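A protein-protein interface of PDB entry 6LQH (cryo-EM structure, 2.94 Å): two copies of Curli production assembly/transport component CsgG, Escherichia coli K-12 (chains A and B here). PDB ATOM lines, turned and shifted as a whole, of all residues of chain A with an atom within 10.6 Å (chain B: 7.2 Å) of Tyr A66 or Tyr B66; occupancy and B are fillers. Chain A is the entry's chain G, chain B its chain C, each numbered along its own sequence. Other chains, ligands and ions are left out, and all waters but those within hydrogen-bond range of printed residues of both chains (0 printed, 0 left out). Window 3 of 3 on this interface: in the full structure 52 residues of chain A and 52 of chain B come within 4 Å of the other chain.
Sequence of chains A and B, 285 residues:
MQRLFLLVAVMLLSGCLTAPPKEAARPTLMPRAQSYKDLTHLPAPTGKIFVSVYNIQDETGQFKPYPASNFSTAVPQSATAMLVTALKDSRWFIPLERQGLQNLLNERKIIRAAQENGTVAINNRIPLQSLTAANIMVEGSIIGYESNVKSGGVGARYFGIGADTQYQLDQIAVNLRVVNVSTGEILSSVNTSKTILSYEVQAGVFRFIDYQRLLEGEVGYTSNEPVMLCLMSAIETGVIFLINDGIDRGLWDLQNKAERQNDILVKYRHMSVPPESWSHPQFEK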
ATOM      1  N   PHE A  63     -21.447  27.654 -11.646  1.00  0.00           N
ATOM      2  CA  PHE A  63     -21.639  26.282 -11.220  1.00  0.00           C
ATOM      3  C   PHE A  63     -23.012  26.167 -10.586  1.00  0.00           C
ATOM      4  O   PHE A  63     -23.756  27.142 -10.494  1.00  0.00           O
ATOM      5  CB  PHE A  63     -20.548  25.840 -10.244  1.00  0.00           C
ATOM      6  CG  PHE A  63     -19.201  25.706 -10.868  1.00  0.00           C
ATOM      7  CD1 PHE A  63     -18.433  26.808 -11.126  1.00  0.00           C
ATOM      8  CD2 PHE A  63     -18.705  24.473 -11.200  1.00  0.00           C
ATOM      9  CE1 PHE A  63     -17.208  26.681 -11.701  1.00  0.00           C
ATOM     10  CE2 PHE A  63     -17.477  24.348 -11.774  1.00  0.00           C
ATOM     11  CZ  PHE A  63     -16.730  25.453 -12.021  1.00  0.00           C
ATOM     12  N   LYS A  64     -23.352  24.966 -10.150  1.00  0.00           N
ATOM     13  CA  LYS A  64     -24.718  24.914  -9.653  1.00  0.00           C
ATOM     14  C   LYS A  64     -24.749  25.136  -8.145  1.00  0.00           C
ATOM     15  O   LYS A  64     -23.810  24.756  -7.442  1.00  0.00           O
ATOM     16  CB  LYS A  64     -25.357  23.575  -9.975  1.00  0.00           C
ATOM     17  CG  LYS A  64     -25.562  23.306 -11.437  1.00  0.00           C
ATOM     18  CD  LYS A  64     -26.264  21.991 -11.624  1.00  0.00           C
ATOM     19  CE  LYS A  64     -27.401  22.108 -12.595  1.00  0.00           C
ATOM     20  NZ  LYS A  64     -26.899  22.316 -13.971  1.00  0.00           N
ATOM     21  N   PRO A  65     -25.812  25.734  -7.623  1.00  0.00           N
ATOM     22  CA  PRO A  65     -25.898  25.951  -6.177  1.00  0.00           C
ATOM     23  C   PRO A  65     -26.225  24.680  -5.417  1.00  0.00           C
ATOM     24  O   PRO A  65     -26.558  23.661  -6.020  1.00  0.00           O
ATOM     25  CB  PRO A  65     -27.023  26.978  -6.052  1.00  0.00           C
ATOM     26  CG  PRO A  65     -27.866  26.727  -7.221  1.00  0.00           C
ATOM     27  CD  PRO A  65     -26.955  26.330  -8.330  1.00  0.00           C
ATOM     28  N   TYR A  66     -26.125  24.736  -4.095  1.00  0.00           N
ATOM     29  CA  TYR A  66     -26.510  23.611  -3.260  1.00  0.00           C
ATOM     30  C   TYR A  66     -27.953  23.214  -3.567  1.00  0.00           C
ATOM     31  O   TYR A  66     -28.781  24.083  -3.859  1.00  0.00           O
ATOM     32  CB  TYR A  66     -26.358  23.992  -1.788  1.00  0.00           C
ATOM     33  CG  TYR A  66     -26.404  22.840  -0.823  1.00  0.00           C
ATOM     34  CD1 TYR A  66     -27.567  22.541  -0.132  1.00  0.00           C
ATOM     35  CD2 TYR A  66     -25.286  22.055  -0.596  1.00  0.00           C
ATOM     36  CE1 TYR A  66     -27.618  21.491   0.747  1.00  0.00           C
ATOM     37  CE2 TYR A  66     -25.327  21.001   0.286  1.00  0.00           C
ATOM     38  CZ  TYR A  66     -26.498  20.723   0.956  1.00  0.00           C
ATOM     39  OH  TYR A  66     -26.554  19.674   1.840  1.00  0.00           O
ATOM     40  N   PRO A  67     -28.299  21.917  -3.508  1.00  0.00           N
ATOM     41  CA  PRO A  67     -27.555  20.729  -3.081  1.00  0.00           C
ATOM     42  C   PRO A  67     -26.584  20.174  -4.100  1.00  0.00           C
ATOM     43  O   PRO A  67     -25.872  19.228  -3.785  1.00  0.00           O
ATOM     44  CB  PRO A  67     -28.659  19.702  -2.820  1.00  0.00           C
ATOM     45  CG  PRO A  67     -29.950  20.437  -2.972  1.00  0.00           C
ATOM     46  CD  PRO A  67     -29.672  21.562  -3.880  1.00  0.00           C
ATOM     47  N   ALA A  68     -26.557  20.742  -5.299  1.00  0.00           N
ATOM     48  CA  ALA A  68     -25.699  20.215  -6.340  1.00  0.00           C
ATOM     49  C   ALA A  68     -24.240  20.266  -5.906  1.00  0.00           C
ATOM     50  O   ALA A  68     -23.862  20.966  -4.968  1.00  0.00           O
ATOM     51  CB  ALA A  68     -25.896  20.990  -7.636  1.00  0.00           C
ATOM     52  N   SER A  69     -23.413  19.496  -6.600  1.00  0.00           N
ATOM     53  CA  SER A  69     -21.999  19.477  -6.286  1.00  0.00           C
ATOM     54  C   SER A  69     -21.374  20.832  -6.583  1.00  0.00           C
ATOM     55  O   SER A  69     -21.884  21.622  -7.378  1.00  0.00           O
ATOM     56  CB  SER A  69     -21.293  18.383  -7.076  1.00  0.00           C
ATOM     57  OG  SER A  69     -19.896  18.563  -7.052  1.00  0.00           O
ATOM     58  N   ASN A  70     -20.258  21.109  -5.917  1.00  0.00           N
ATOM     59  CA  ASN A  70     -19.569  22.367  -6.156  1.00  0.00           C
ATOM     60  C   ASN A  70     -18.916  22.408  -7.525  1.00  0.00           C
ATOM     61  O   ASN A  70     -18.664  23.499  -8.042  1.00  0.00           O
ATOM     62  CB  ASN A  70     -18.518  22.606  -5.082  1.00  0.00           C
ATOM     63  CG  ASN A  70     -19.123  22.997  -3.766  1.00  0.00           C
ATOM     64  OD1 ASN A  70     -19.419  24.165  -3.529  1.00  0.00           O
ATOM     65  ND2 ASN A  70     -19.314  22.021  -2.893  1.00  0.00           N
ATOM     66  N   PHE A  71     -18.636  21.254  -8.117  1.00  0.00           N
ATOM     67  CA  PHE A  71     -17.958  21.169  -9.397  1.00  0.00           C
ATOM     68  C   PHE A  71     -18.918  20.974 -10.552  1.00  0.00           C
ATOM     69  O   PHE A  71     -18.475  20.818 -11.691  1.00  0.00           O
ATOM     70  CB  PHE A  71     -16.946  20.027  -9.377  1.00  0.00           C
ATOM     71  CG  PHE A  71     -16.061  20.029  -8.178  1.00  0.00           C
ATOM     72  CD1 PHE A  71     -14.919  20.797  -8.150  1.00  0.00           C
ATOM     73  CD2 PHE A  71     -16.367  19.263  -7.079  1.00  0.00           C
ATOM     74  CE1 PHE A  71     -14.106  20.802  -7.053  1.00  0.00           C
ATOM     75  CE2 PHE A  71     -15.556  19.269  -5.979  1.00  0.00           C
ATOM     76  CZ  PHE A  71     -14.426  20.037  -5.967  1.00  0.00           C
ATOM     77  N   SER A  72     -20.216  20.975 -10.287  1.00  0.00           N
ATOM     78  CA  SER A  72     -21.215  20.720 -11.310  1.00  0.00           C
ATOM     79  C   SER A  72     -21.574  22.035 -11.981  1.00  0.00           C
ATOM     80  O   SER A  72     -22.284  22.856 -11.401  1.00  0.00           O
ATOM     81  CB  SER A  72     -22.431  20.056 -10.681  1.00  0.00           C
ATOM     82  OG  SER A  72     -23.600  20.379 -11.386  1.00  0.00           O
ATOM     83  N   ALA A  74     -23.144  24.981 -14.337  1.00  0.00           N
ATOM     84  CA  ALA A  74     -24.529  25.322 -14.608  1.00  0.00           C
ATOM     85  C   ALA A  74     -24.906  25.086 -16.056  1.00  0.00           C
ATOM     86  O   ALA A  74     -26.090  24.908 -16.357  1.00  0.00           O
ATOM     87  CB  ALA A  74     -24.788  26.780 -14.252  1.00  0.00           C
ATOM     88  N   SER A 147     -28.898  32.577 -12.908  1.00  0.00           N
ATOM     89  CA  SER A 147     -29.841  31.728 -12.205  1.00  0.00           C
ATOM     90  C   SER A 147     -30.897  32.596 -11.547  1.00  0.00           C
ATOM     91  O   SER A 147     -30.568  33.498 -10.772  1.00  0.00           O
ATOM     92  CB  SER A 147     -29.122  30.873 -11.164  1.00  0.00           C
ATOM     93  OG  SER A 147     -30.038  30.284 -10.258  1.00  0.00           O
ATOM     94  N   ASN A 148     -32.158  32.318 -11.857  1.00  0.00           N
ATOM     95  CA  ASN A 148     -33.304  33.030 -11.298  1.00  0.00           C
ATOM     96  C   ASN A 148     -33.265  34.512 -11.652  1.00  0.00           C
ATOM     97  O   ASN A 148     -33.171  35.380 -10.787  1.00  0.00           O
ATOM     98  CB  ASN A 148     -33.382  32.851  -9.783  1.00  0.00           C
ATOM     99  CG  ASN A 148     -33.384  31.408  -9.377  1.00  0.00           C
ATOM    100  OD1 ASN A 148     -34.006  30.576 -10.031  1.00  0.00           O
ATOM    101  ND2 ASN A 148     -32.695  31.095  -8.291  1.00  0.00           N
ATOM    102  N   GLN A 168     -39.231  29.643 -11.867  1.00  0.00           N
ATOM    103  CA  GLN A 168     -37.933  30.284 -11.928  1.00  0.00           C
ATOM    104  C   GLN A 168     -37.538  30.390 -13.385  1.00  0.00           C
ATOM    105  O   GLN A 168     -37.746  29.458 -14.158  1.00  0.00           O
ATOM    106  CB  GLN A 168     -36.871  29.499 -11.168  1.00  0.00           C
ATOM    107  CG  GLN A 168     -37.030  29.536  -9.676  1.00  0.00           C
ATOM    108  CD  GLN A 168     -36.023  28.664  -8.972  1.00  0.00           C
ATOM    109  OE1 GLN A 168     -35.110  28.131  -9.594  1.00  0.00           O
ATOM    110  NE2 GLN A 168     -36.183  28.512  -7.666  1.00  0.00           N
ATOM    111  N   LYS B  64     -22.758  14.596  -9.048  1.00  0.00           N
ATOM    112  CA  LYS B  64     -24.019  14.241  -8.414  1.00  0.00           C
ATOM    113  C   LYS B  64     -24.291  15.144  -7.216  1.00  0.00           C
ATOM    114  O   LYS B  64     -23.356  15.587  -6.548  1.00  0.00           O
ATOM    115  CB  LYS B  64     -24.002  12.794  -7.956  1.00  0.00           C
ATOM    116  CG  LYS B  64     -23.927  11.781  -9.060  1.00  0.00           C
ATOM    117  CD  LYS B  64     -23.990  10.392  -8.488  1.00  0.00           C
ATOM    118  CE  LYS B  64     -24.968   9.534  -9.234  1.00  0.00           C
ATOM    119  NZ  LYS B  64     -24.464   9.219 -10.590  1.00  0.00           N
ATOM    120  N   PRO B  65     -25.553  15.424  -6.918  1.00  0.00           N
ATOM    121  CA  PRO B  65     -25.865  16.269  -5.764  1.00  0.00           C
ATOM    122  C   PRO B  65     -25.703  15.538  -4.445  1.00  0.00           C
ATOM    123  O   PRO B  65     -25.516  14.321  -4.426  1.00  0.00           O
ATOM    124  CB  PRO B  65     -27.324  16.654  -6.008  1.00  0.00           C
ATOM    125  CG  PRO B  65     -27.863  15.538  -6.785  1.00  0.00           C
ATOM    126  CD  PRO B  65     -26.763  15.059  -7.668  1.00  0.00           C
ATOM    127  N   TYR B  66     -25.768  16.276  -3.345  1.00  0.00           N
ATOM    128  CA  TYR B  66     -25.727  15.668  -2.025  1.00  0.00           C
ATOM    129  C   TYR B  66     -26.831  14.620  -1.907  1.00  0.00           C
ATOM    130  O   TYR B  66     -27.914  14.800  -2.474  1.00  0.00           O
ATOM    131  CB  TYR B  66     -25.897  16.751  -0.960  1.00  0.00           C
ATOM    132  CG  TYR B  66     -25.552  16.328   0.441  1.00  0.00           C
ATOM    133  CD1 TYR B  66     -26.544  15.962   1.335  1.00  0.00           C
ATOM    134  CD2 TYR B  66     -24.236  16.298   0.873  1.00  0.00           C
ATOM    135  CE1 TYR B  66     -26.238  15.572   2.614  1.00  0.00           C
ATOM    136  CE2 TYR B  66     -23.918  15.910   2.153  1.00  0.00           C
ATOM    137  CZ  TYR B  66     -24.925  15.548   3.020  1.00  0.00           C
ATOM    138  OH  TYR B  66     -24.624  15.159   4.302  1.00  0.00           O
ATOM    139  N   PRO B  67     -26.605  13.514  -1.180  1.00  0.00           N
ATOM    140  CA  PRO B  67     -25.478  13.121  -0.329  1.00  0.00           C
ATOM    141  C   PRO B  67     -24.268  12.591  -1.066  1.00  0.00           C
ATOM    142  O   PRO B  67     -23.260  12.315  -0.425  1.00  0.00           O
ATOM    143  CB  PRO B  67     -26.069  12.009   0.543  1.00  0.00           C
ATOM    144  CG  PRO B  67     -27.528  11.966   0.222  1.00  0.00           C
ATOM    145  CD  PRO B  67     -27.657  12.494  -1.146  1.00  0.00           C
ATOM    146  N   ALA B  68     -24.362  12.444  -2.381  1.00  0.00           N
ATOM    147  CA  ALA B  68     -23.262  11.878  -3.136  1.00  0.00           C
ATOM    148  C   ALA B  68     -22.011  12.732  -2.977  1.00  0.00           C
ATOM    149  O   ALA B  68     -22.058  13.888  -2.557  1.00  0.00           O
ATOM    150  CB  ALA B  68     -23.635  11.750  -4.606  1.00  0.00           C
ATOM    151  N   SER B  69     -20.872  12.139  -3.309  1.00  0.00           N
ATOM    152  CA  SER B  69     -19.620  12.861  -3.214  1.00  0.00           C
ATOM    153  C   SER B  69     -19.596  14.008  -4.214  1.00  0.00           C
ATOM    154  O   SER B  69     -20.308  14.010  -5.217  1.00  0.00           O
ATOM    155  CB  SER B  69     -18.446  11.923  -3.456  1.00  0.00           C
ATOM    156  OG  SER B  69     -17.262  12.647  -3.706  1.00  0.00           O
ATOM    157  N   ASN B  70     -18.771  15.009  -3.919  1.00  0.00           N
ATOM    158  CA  ASN B  70     -18.653  16.137  -4.829  1.00  0.00           C
ATOM    159  C   ASN B  70     -17.946  15.760  -6.116  1.00  0.00           C
ATOM    160  O   ASN B  70     -18.125  16.443  -7.127  1.00  0.00           O
ATOM    161  CB  ASN B  70     -17.913  17.284  -4.155  1.00  0.00           C
ATOM    162  CG  ASN B  70     -18.756  17.986  -3.131  1.00  0.00           C
ATOM    163  OD1 ASN B  70     -19.536  18.875  -3.456  1.00  0.00           O
ATOM    164  ND2 ASN B  70     -18.604  17.592  -1.877  1.00  0.00           N
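Printed residues of chain A that touch a printed residue of chain B: Tyr A66, Pro A67, Ala A68, Ser A69, Asn A70 and Phe A71.
Hydrophobic or aromatic side chains of chain A that line the printed part of chain B: Tyr A66 and Phe A71.
Hydrophobic or aromatic side chains of chain B within 4 Å of the printed part of chain A: Pro B65 and Tyr B66.
Among the printed residues, 8 pairs touch across the chains.
Among the printed residues, no Asp or Glu carboxylate lies within 4 Å of a Lys or Arg side-chain nitrogen of the other chain.
Pro A67 touches Tyr B66, but with the chains exchanged Tyr A66 does not touch Pro B67 (6.9 Å).
Ala A68 touches Pro B65, but with the chains exchanged Pro A65 does not touch Ala B68 (11.3 Å).
Ser A69 touches Lys B64, but with the chains exchanged Lys A64 does not touch Ser B69 (11.5 Å).
Ser A69 touches Asn B70, but with the chains exchanged Asn A70 does not touch Ser B69 (7.1 Å).
Positions printed for both chains: 64, 65, 66, 67, 68, 69 and 70.
The side-chain hydroxyl of Ser A69 is in hydrogen-bond range of the backbone NH of Phe A71 (3.2 Å).
Pro A65 touches none of the printed residues of chain B.
Of the printed residues of chain B, Pro A67 touches Pro B65 and Tyr B66.
Printed residues of chain B within 4 Å of Ala A68: Pro B65 (3.9 Å).
Of the printed residues of chain B, Ser A69 touches Lys B64 (3.5 Å) and Asn B70 (2.8 Å).
Printed residues of chain B within 4 Å of Phe A71: Asn B70 (3.3 Å).
Printed residues of chain A within 4 Å of Lys B64: Ser A69 (3.5 Å).
Of chain A, only Pro A67 (3.6 Å) and Ala A68 (3.9 Å) come within 4 Å of Pro B65.
No residue of chain A comes within 4 Å of Pro B67.
The nearest residue of chain A that does not touch Tyr B66 is Ala A68 (4.9 Å).
The nearest printed residue of chain B that does not touch Pro A67 is Lys B64 (5.2 Å).
OH of Tyr A66 touches CD1 of Tyr B66 (3.7 Å).
CA of Pro B65 touches O of Pro A67, 3.6 Å away.
CA of Ala A68 touches CB of Pro B65, 3.9 Å away.
Ser A69 touches Lys B64 (CB to O, 3.5 Å).
Asn B70 touches Phe A71.
ND2 of Asn A70 lies within hydrogen-bond range of OD1 of Asn B70.
The backbone NH of Tyr B66 lies within hydrogen-bond range of the backbone carbonyl oxygen of Pro A67, 3.0 Å away.
O of Asn B70 lies within hydrogen-bond range of OG of Ser A69 (2.8 Å).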
